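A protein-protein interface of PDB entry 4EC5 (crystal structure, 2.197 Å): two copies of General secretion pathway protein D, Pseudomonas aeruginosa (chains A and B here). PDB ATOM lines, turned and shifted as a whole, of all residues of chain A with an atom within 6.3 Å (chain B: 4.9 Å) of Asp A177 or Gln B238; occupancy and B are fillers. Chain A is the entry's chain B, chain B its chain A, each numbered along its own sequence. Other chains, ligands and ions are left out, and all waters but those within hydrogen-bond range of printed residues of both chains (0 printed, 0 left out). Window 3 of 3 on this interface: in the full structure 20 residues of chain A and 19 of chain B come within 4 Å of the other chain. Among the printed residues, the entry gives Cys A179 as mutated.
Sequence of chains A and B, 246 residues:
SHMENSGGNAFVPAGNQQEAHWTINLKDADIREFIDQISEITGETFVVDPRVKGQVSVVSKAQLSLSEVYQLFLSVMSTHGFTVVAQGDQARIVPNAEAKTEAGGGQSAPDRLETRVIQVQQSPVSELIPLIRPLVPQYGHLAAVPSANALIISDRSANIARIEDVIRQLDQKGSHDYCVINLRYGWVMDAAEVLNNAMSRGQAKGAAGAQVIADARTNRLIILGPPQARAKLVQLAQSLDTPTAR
Of the 12 printed residues of chain B, 4 touch a printed residue of chain A.
Hydrophobic or aromatic side chains of chain B within 4 Å of the printed part of chain A: Val B180 and Ile B181.
Of the 11 printed residues of chain A, 4 touch a printed residue of chain B.
Among the printed residues, 7 pairs touch across the chains.
Among the printed residues, no Asp or Glu carboxylate lies within 4 Å of a Lys or Arg side-chain nitrogen of the other chain.
N of His A176 sits at hydrogen-bond distance from OE1 of Glu A127 (2.8 Å).
The backbone carbonyl oxygen (O) of Ser A175 is in hydrogen-bond range of the side-chain amide nitrogen (NE2) of Gln A172.
The side-chain amide nitrogen (NE2) of Gln A172 sits close to a ring nitrogen (NE2) of His A176, at 3.5 Å.
The guanidinium group (NE) of Arg A230 lies within hydrogen-bond range of the backbone carbonyl oxygen (O) of Asp A177, 3.4 Å away.
Of chain B, only Val B180 (3.4 Å), Ile B181 (3.6 Å), Asn B182 (2.7 Å) and Gln B238 (3.6 Å) come within 4 Å of Asp A177.
Gln B238 touches one residue of chain A.
Of the printed residues of chain A, Val B180 touches Asp A177 and Tyr A178.
Of the printed residues of chain B, His A176 touches Asn B182 (3.1 Å).
Of the printed residues of chain A, Asn B182 touches Ser A175 (3.7 Å), His A176 (3.1 Å) and Asp A177 (2.7 Å).
Printed residues of chain B within 4 Å of Tyr A178: Val B180.
Printed residues of chain B within 4 Å of Ser A175: Asn B182.
Gln B235 touches none of the printed residues of chain A.
The nearest printed residue of chain B that does not touch Asp A177 is Val B234 (6.8 Å).
No position is printed for both chains.
The backbone NH (N) of Val B180 lies within hydrogen-bond range of the backbone carbonyl oxygen (O) of Tyr A178 (2.7 Å).
The side-chain amide nitrogen (ND2) of Asn B182 is in hydrogen-bond range of the backbone carbonyl oxygen (O) of His A176 (3.1 Å).
The side-chain carboxylate (OD1) of Asp A177 sits at hydrogen-bond distance from the side-chain amide nitrogen (ND2) of Asn B182 (2.7 Å).
Among the printed residues, pairs that only touch across the chains: Ser A175 with Asn B182, Asp A177 with Val B180, Asp A177 with Ile B181 and Asp A177 with Gln B238.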
ATOM      1  N   GLU A 127       3.190  -4.778  30.620  1.00  0.00           N
ATOM      2  CA  GLU A 127       1.749  -4.986  30.472  1.00  0.00           C
ATOM      3  C   GLU A 127       1.337  -6.463  30.383  1.00  0.00           C
ATOM      4  O   GLU A 127       0.350  -6.868  30.963  1.00  0.00           O
ATOM      5  CB  GLU A 127       1.187  -4.200  29.286  1.00  0.00           C
ATOM      6  CG  GLU A 127      -0.317  -4.382  29.112  1.00  0.00           C
ATOM      7  CD  GLU A 127      -0.976  -3.390  28.155  1.00  0.00           C
ATOM      8  OE1 GLU A 127      -2.191  -3.171  28.277  1.00  0.00           O
ATOM      9  OE2 GLU A 127      -0.286  -2.831  27.289  1.00  0.00           O
ATOM     10  N   GLN A 172       0.504  -6.803  20.448  1.00  0.00           N
ATOM     11  CA  GLN A 172      -0.155  -5.752  19.668  1.00  0.00           C
ATOM     12  C   GLN A 172       0.339  -4.381  20.131  1.00  0.00           C
ATOM     13  O   GLN A 172       0.851  -4.252  21.246  1.00  0.00           O
ATOM     14  CB  GLN A 172      -1.680  -5.828  19.779  1.00  0.00           C
ATOM     15  CG  GLN A 172      -2.190  -5.456  21.163  1.00  0.00           C
ATOM     16  CD  GLN A 172      -3.687  -5.627  21.316  1.00  0.00           C
ATOM     17  OE1 GLN A 172      -4.308  -6.452  20.642  1.00  0.00           O
ATOM     18  NE2 GLN A 172      -4.278  -4.831  22.200  1.00  0.00           N
ATOM     19  N   SER A 175      -2.945  -0.859  23.891  1.00  0.00           N
ATOM     20  CA  SER A 175      -3.093  -1.405  25.240  1.00  0.00           C
ATOM     21  C   SER A 175      -4.202  -2.447  25.288  1.00  0.00           C
ATOM     22  O   SER A 175      -5.122  -2.429  24.472  1.00  0.00           O
ATOM     23  CB  SER A 175      -3.400  -0.281  26.227  1.00  0.00           C
ATOM     24  OG  SER A 175      -2.358   0.672  26.244  1.00  0.00           O
ATOM     25  N   HIS A 176      -4.104  -3.349  26.258  1.00  0.00           N
ATOM     26  CA  HIS A 176      -5.082  -4.418  26.423  1.00  0.00           C
ATOM     27  C   HIS A 176      -6.120  -4.111  27.501  1.00  0.00           C
ATOM     28  O   HIS A 176      -5.853  -4.290  28.692  1.00  0.00           O
ATOM     29  CB  HIS A 176      -4.387  -5.743  26.743  1.00  0.00           C
ATOM     30  CG  HIS A 176      -4.091  -6.578  25.537  1.00  0.00           C
ATOM     31  ND1 HIS A 176      -5.076  -7.166  24.772  1.00  0.00           N
ATOM     32  CD2 HIS A 176      -2.914  -6.913  24.960  1.00  0.00           C
ATOM     33  CE1 HIS A 176      -4.517  -7.835  23.780  1.00  0.00           C
ATOM     34  NE2 HIS A 176      -3.207  -7.696  23.871  1.00  0.00           N
ATOM     35  N   ASP A 177      -7.300  -3.651  27.094  1.00  0.00           N
ATOM     36  CA  ASP A 177      -8.403  -3.528  28.030  1.00  0.00           C
ATOM     37  C   ASP A 177      -8.876  -4.957  28.250  1.00  0.00           C
ATOM     38  O   ASP A 177      -8.791  -5.783  27.340  1.00  0.00           O
ATOM     39  CB  ASP A 177      -9.547  -2.711  27.430  1.00  0.00           C
ATOM     40  CG  ASP A 177      -9.285  -1.216  27.472  1.00  0.00           C
ATOM     41  OD1 ASP A 177      -8.217  -0.811  27.973  1.00  0.00           O
ATOM     42  OD2 ASP A 177     -10.148  -0.447  26.996  1.00  0.00           O
ATOM     43  N   TYR A 178      -9.381  -5.258  29.442  1.00  0.00           N
ATOM     44  CA  TYR A 178      -9.884  -6.603  29.698  1.00  0.00           C
ATOM     45  C   TYR A 178     -10.924  -6.692  30.803  1.00  0.00           C
ATOM     46  O   TYR A 178     -11.126  -5.752  31.565  1.00  0.00           O
ATOM     47  CB  TYR A 178      -8.721  -7.551  30.010  1.00  0.00           C
ATOM     48  CG  TYR A 178      -7.908  -7.195  31.236  1.00  0.00           C
ATOM     49  CD1 TYR A 178      -8.228  -7.718  32.482  1.00  0.00           C
ATOM     50  CD2 TYR A 178      -6.789  -6.384  31.135  1.00  0.00           C
ATOM     51  CE1 TYR A 178      -7.469  -7.417  33.597  1.00  0.00           C
ATOM     52  CE2 TYR A 178      -6.026  -6.071  32.243  1.00  0.00           C
ATOM     53  CZ  TYR A 178      -6.369  -6.594  33.471  1.00  0.00           C
ATOM     54  OH  TYR A 178      -5.620  -6.277  34.580  1.00  0.00           O
ATOM     55  N   CYS A 179     -11.572  -7.850  30.869  1.00  0.00           N
ATOM     56  CA  CYS A 179     -12.581  -8.119  31.884  1.00  0.00           C
ATOM     57  C   CYS A 179     -12.237  -9.397  32.649  1.00  0.00           C
ATOM     58  O   CYS A 179     -11.765 -10.372  32.069  1.00  0.00           O
ATOM     59  CB  CYS A 179     -13.964  -8.229  31.242  1.00  0.00           C
ATOM     60  SG  CYS A 179     -14.659  -6.638  30.716  1.00  0.00           S
ATOM     61  N   ILE A 223     -10.722 -11.955  30.006  1.00  0.00           N
ATOM     62  CA  ILE A 223     -11.226 -11.806  28.663  1.00  0.00           C
ATOM     63  C   ILE A 223     -10.666 -10.560  27.966  1.00  0.00           C
ATOM     64  O   ILE A 223     -10.861  -9.447  28.422  1.00  0.00           O
ATOM     65  CB  ILE A 223     -12.754 -11.676  28.662  1.00  0.00           C
ATOM     66  CG1 ILE A 223     -13.401 -12.703  29.602  1.00  0.00           C
ATOM     67  CG2 ILE A 223     -13.276 -11.764  27.249  1.00  0.00           C
ATOM     68  CD1 ILE A 223     -13.534 -14.069  29.076  1.00  0.00           C
ATOM     69  N   LEU A 224     -10.045 -10.767  26.816  1.00  0.00           N
ATOM     70  CA  LEU A 224      -9.325  -9.739  26.086  1.00  0.00           C
ATOM     71  C   LEU A 224      -9.934  -9.545  24.711  1.00  0.00           C
ATOM     72  O   LEU A 224     -10.745 -10.339  24.277  1.00  0.00           O
ATOM     73  CB  LEU A 224      -7.866 -10.135  25.871  1.00  0.00           C
ATOM     74  CG  LEU A 224      -6.829 -10.470  26.954  1.00  0.00           C
ATOM     75  CD1 LEU A 224      -6.486  -9.231  27.733  1.00  0.00           C
ATOM     76  CD2 LEU A 224      -7.283 -11.584  27.850  1.00  0.00           C
ATOM     77  N   GLY A 225      -9.545  -8.466  24.045  1.00  0.00           N
ATOM     78  CA  GLY A 225      -9.822  -8.289  22.630  1.00  0.00           C
ATOM     79  C   GLY A 225     -10.360  -6.907  22.299  1.00  0.00           C
ATOM     80  O   GLY A 225     -10.468  -6.053  23.179  1.00  0.00           O
ATOM     81  N   ARG A 230     -14.828  -8.598  22.596  1.00  0.00           N
ATOM     82  CA  ARG A 230     -14.600  -8.781  24.024  1.00  0.00           C
ATOM     83  C   ARG A 230     -15.898  -8.738  24.819  1.00  0.00           C
ATOM     84  O   ARG A 230     -16.147  -9.607  25.658  1.00  0.00           O
ATOM     85  CB  ARG A 230     -13.617  -7.716  24.525  1.00  0.00           C
ATOM     86  CG  ARG A 230     -13.506  -7.598  26.039  1.00  0.00           C
ATOM     87  CD  ARG A 230     -12.187  -6.952  26.462  1.00  0.00           C
ATOM     88  NE  ARG A 230     -11.722  -5.906  25.550  1.00  0.00           N
ATOM     89  CZ  ARG A 230     -12.072  -4.625  25.605  1.00  0.00           C
ATOM     90  NH1 ARG A 230     -12.891  -4.179  26.548  1.00  0.00           N
ATOM     91  NH2 ARG A 230     -11.597  -3.779  24.700  1.00  0.00           N
ATOM     92  N   VAL B 180     -11.140  -3.486  33.088  1.00  0.00           N
ATOM     93  CA  VAL B 180     -10.040  -2.530  33.116  1.00  0.00           C
ATOM     94  C   VAL B 180     -10.054  -1.677  31.853  1.00  0.00           C
ATOM     95  O   VAL B 180     -10.163  -2.203  30.744  1.00  0.00           O
ATOM     96  CB  VAL B 180      -8.696  -3.267  33.270  1.00  0.00           C
ATOM     97  CG1 VAL B 180      -7.533  -2.297  33.142  1.00  0.00           C
ATOM     98  CG2 VAL B 180      -8.641  -3.995  34.609  1.00  0.00           C
ATOM     99  N   ILE B 181      -9.944  -0.365  32.024  1.00  0.00           N
ATOM    100  CA  ILE B 181      -9.897   0.542  30.885  1.00  0.00           C
ATOM    101  C   ILE B 181      -8.629   1.385  30.911  1.00  0.00           C
ATOM    102  O   ILE B 181      -8.419   2.186  31.821  1.00  0.00           O
ATOM    103  CB  ILE B 181     -11.127   1.482  30.834  1.00  0.00           C
ATOM    104  CG1 ILE B 181     -12.432   0.683  30.785  1.00  0.00           C
ATOM    105  CG2 ILE B 181     -11.043   2.411  29.628  1.00  0.00           C
ATOM    106  CD1 ILE B 181     -13.661   1.532  31.065  1.00  0.00           C
ATOM    107  N   ASN B 182      -7.795   1.202  29.890  1.00  0.00           N
ATOM    108  CA  ASN B 182      -6.560   1.961  29.746  1.00  0.00           C
ATOM    109  C   ASN B 182      -6.837   3.249  28.986  1.00  0.00           C
ATOM    110  O   ASN B 182      -7.104   3.225  27.784  1.00  0.00           O
ATOM    111  CB  ASN B 182      -5.554   1.131  28.950  1.00  0.00           C
ATOM    112  CG  ASN B 182      -5.207  -0.176  29.637  1.00  0.00           C
ATOM    113  OD1 ASN B 182      -4.397  -0.208  30.562  1.00  0.00           O
ATOM    114  ND2 ASN B 182      -5.814  -1.266  29.177  1.00  0.00           N
ATOM    115  N   VAL B 234     -18.759   0.865  32.104  1.00  0.00           N
ATOM    116  CA  VAL B 234     -17.651   0.715  31.162  1.00  0.00           C
ATOM    117  C   VAL B 234     -17.878   1.532  29.895  1.00  0.00           C
ATOM    118  O   VAL B 234     -16.972   2.210  29.407  1.00  0.00           O
ATOM    119  CB  VAL B 234     -17.350  -0.760  30.826  1.00  0.00           C
ATOM    120  CG1 VAL B 234     -16.358  -0.849  29.670  1.00  0.00           C
ATOM    121  CG2 VAL B 234     -16.809  -1.482  32.048  1.00  0.00           C
ATOM    122  N   GLN B 235     -19.097   1.474  29.368  1.00  0.00           N
ATOM    123  CA  GLN B 235     -19.467   2.230  28.182  1.00  0.00           C
ATOM    124  C   GLN B 235     -19.389   3.723  28.434  1.00  0.00           C
ATOM    125  O   GLN B 235     -18.905   4.471  27.623  1.00  0.00           O
ATOM    126  CB  GLN B 235     -20.889   1.877  27.738  1.00  0.00           C
ATOM    127  CG  GLN B 235     -21.105   0.442  27.278  1.00  0.00           C
ATOM    128  CD  GLN B 235     -22.577   0.034  27.285  1.00  0.00           C
ATOM    129  OE1 GLN B 235     -23.458   0.850  27.029  1.00  0.00           O
ATOM    130  NE2 GLN B 235     -22.842  -1.234  27.579  1.00  0.00           N
ATOM    131  N   LEU B 236     -19.881   4.144  29.578  1.00  0.00           N
ATOM    132  CA  LEU B 236     -19.803   5.540  29.988  1.00  0.00           C
ATOM    133  C   LEU B 236     -18.353   6.003  30.129  1.00  0.00           C
ATOM    134  O   LEU B 236     -17.990   7.089  29.676  1.00  0.00           O
ATOM    135  CB  LEU B 236     -20.530   5.749  31.317  1.00  0.00           C
ATOM    136  CG  LEU B 236     -20.717   7.205  31.744  1.00  0.00           C
ATOM    137  CD1 LEU B 236     -21.661   7.937  30.807  1.00  0.00           C
ATOM    138  CD2 LEU B 236     -21.242   7.255  33.168  1.00  0.00           C
ATOM    139  N   ALA B 237     -17.530   5.169  30.759  1.00  0.00           N
ATOM    140  CA  ALA B 237     -16.108   5.457  30.920  1.00  0.00           C
ATOM    141  C   ALA B 237     -15.404   5.610  29.575  1.00  0.00           C
ATOM    142  O   ALA B 237     -14.527   6.464  29.422  1.00  0.00           O
ATOM    143  CB  ALA B 237     -15.440   4.365  31.741  1.00  0.00           C
ATOM    144  N   GLN B 238     -15.791   4.803  28.597  1.00  0.00           N
ATOM    145  CA  GLN B 238     -15.207   4.886  27.268  1.00  0.00           C
ATOM    146  C   GLN B 238     -15.482   6.241  26.631  1.00  0.00           C
ATOM    147  O   GLN B 238     -14.642   6.785  25.943  1.00  0.00           O
ATOM    148  CB  GLN B 238     -15.701   3.768  26.369  1.00  0.00           C
ATOM    149  CG  GLN B 238     -15.325   2.379  26.819  1.00  0.00           C
ATOM    150  CD  GLN B 238     -13.840   2.153  26.909  1.00  0.00           C
ATOM    151  OE1 GLN B 238     -13.053   3.000  26.516  1.00  0.00           O
ATOM    152  NE2 GLN B 238     -13.450   0.993  27.416  1.00  0.00           N
ATOM    153  N   SER B 239     -16.668   6.782  26.860  1.00  0.00           N
ATOM    154  CA  SER B 239     -17.045   8.086  26.323  1.00  0.00           C
ATOM    155  C   SER B 239     -16.222   9.255  26.860  1.00  0.00           C
ATOM    156  O   SER B 239     -16.169  10.314  26.236  1.00  0.00           O
ATOM    157  CB  SER B 239     -18.533   8.351  26.541  1.00  0.00           C
ATOM    158  OG  SER B 239     -18.782   8.764  27.876  1.00  0.00           O
ATOM    159  N   LEU B 240     -15.585   9.076  28.012  1.00  0.00           N
ATOM    160  CA  LEU B 240     -14.749  10.135  28.558  1.00  0.00           C
ATOM    161  C   LEU B 240     -13.364  10.077  27.926  1.00  0.00           C
ATOM    162  O   LEU B 240     -12.605  11.043  27.980  1.00  0.00           O
ATOM    163  CB  LEU B 240     -14.635  10.022  30.080  1.00  0.00           C
ATOM    164  CG  LEU B 240     -15.959   9.998  30.852  1.00  0.00           C
ATOM    165  CD1 LEU B 240     -15.717   9.888  32.352  1.00  0.00           C
ATOM    166  CD2 LEU B 240     -16.805  11.226  30.543  1.00  0.00           C
ATOM    167  N   ASP B 241     -13.042   8.937  27.318  1.00  0.00           N
ATOM    168  CA  ASP B 241     -11.763   8.772  26.639  1.00  0.00           C
ATOM    169  C   ASP B 241     -11.885   8.774  25.112  1.00  0.00           C
ATOM    170  O   ASP B 241     -11.190   8.001  24.446  1.00  0.00           O
ATOM    171  CB  ASP B 241     -11.114   7.469  27.114  1.00  0.00           C
ATOM    172  CG  ASP B 241      -9.626   7.423  26.815  1.00  0.00           C
ATOM    173  OD1 ASP B 241      -8.933   8.425  27.086  1.00  0.00           O
ATOM    174  OD2 ASP B 241      -9.149   6.386  26.309  1.00  0.00           O
ATOM    175  N   THR B 242     -12.750   9.609  24.539  1.00  0.00           N
ATOM    176  CA  THR B 242     -12.885   9.611  23.081  1.00  0.00           C
ATOM    177  C   THR B 242     -11.979  10.696  22.520  1.00  0.00           C
ATOM    178  O   THR B 242     -11.859  11.772  23.102  1.00  0.00           O
ATOM    179  CB  THR B 242     -14.353   9.833  22.632  1.00  0.00           C
ATOM    180  OG1 THR B 242     -14.683  11.227  22.709  1.00  0.00           O
ATOM    181  CG2 THR B 242     -15.334   9.015  23.456  1.00  0.00           C
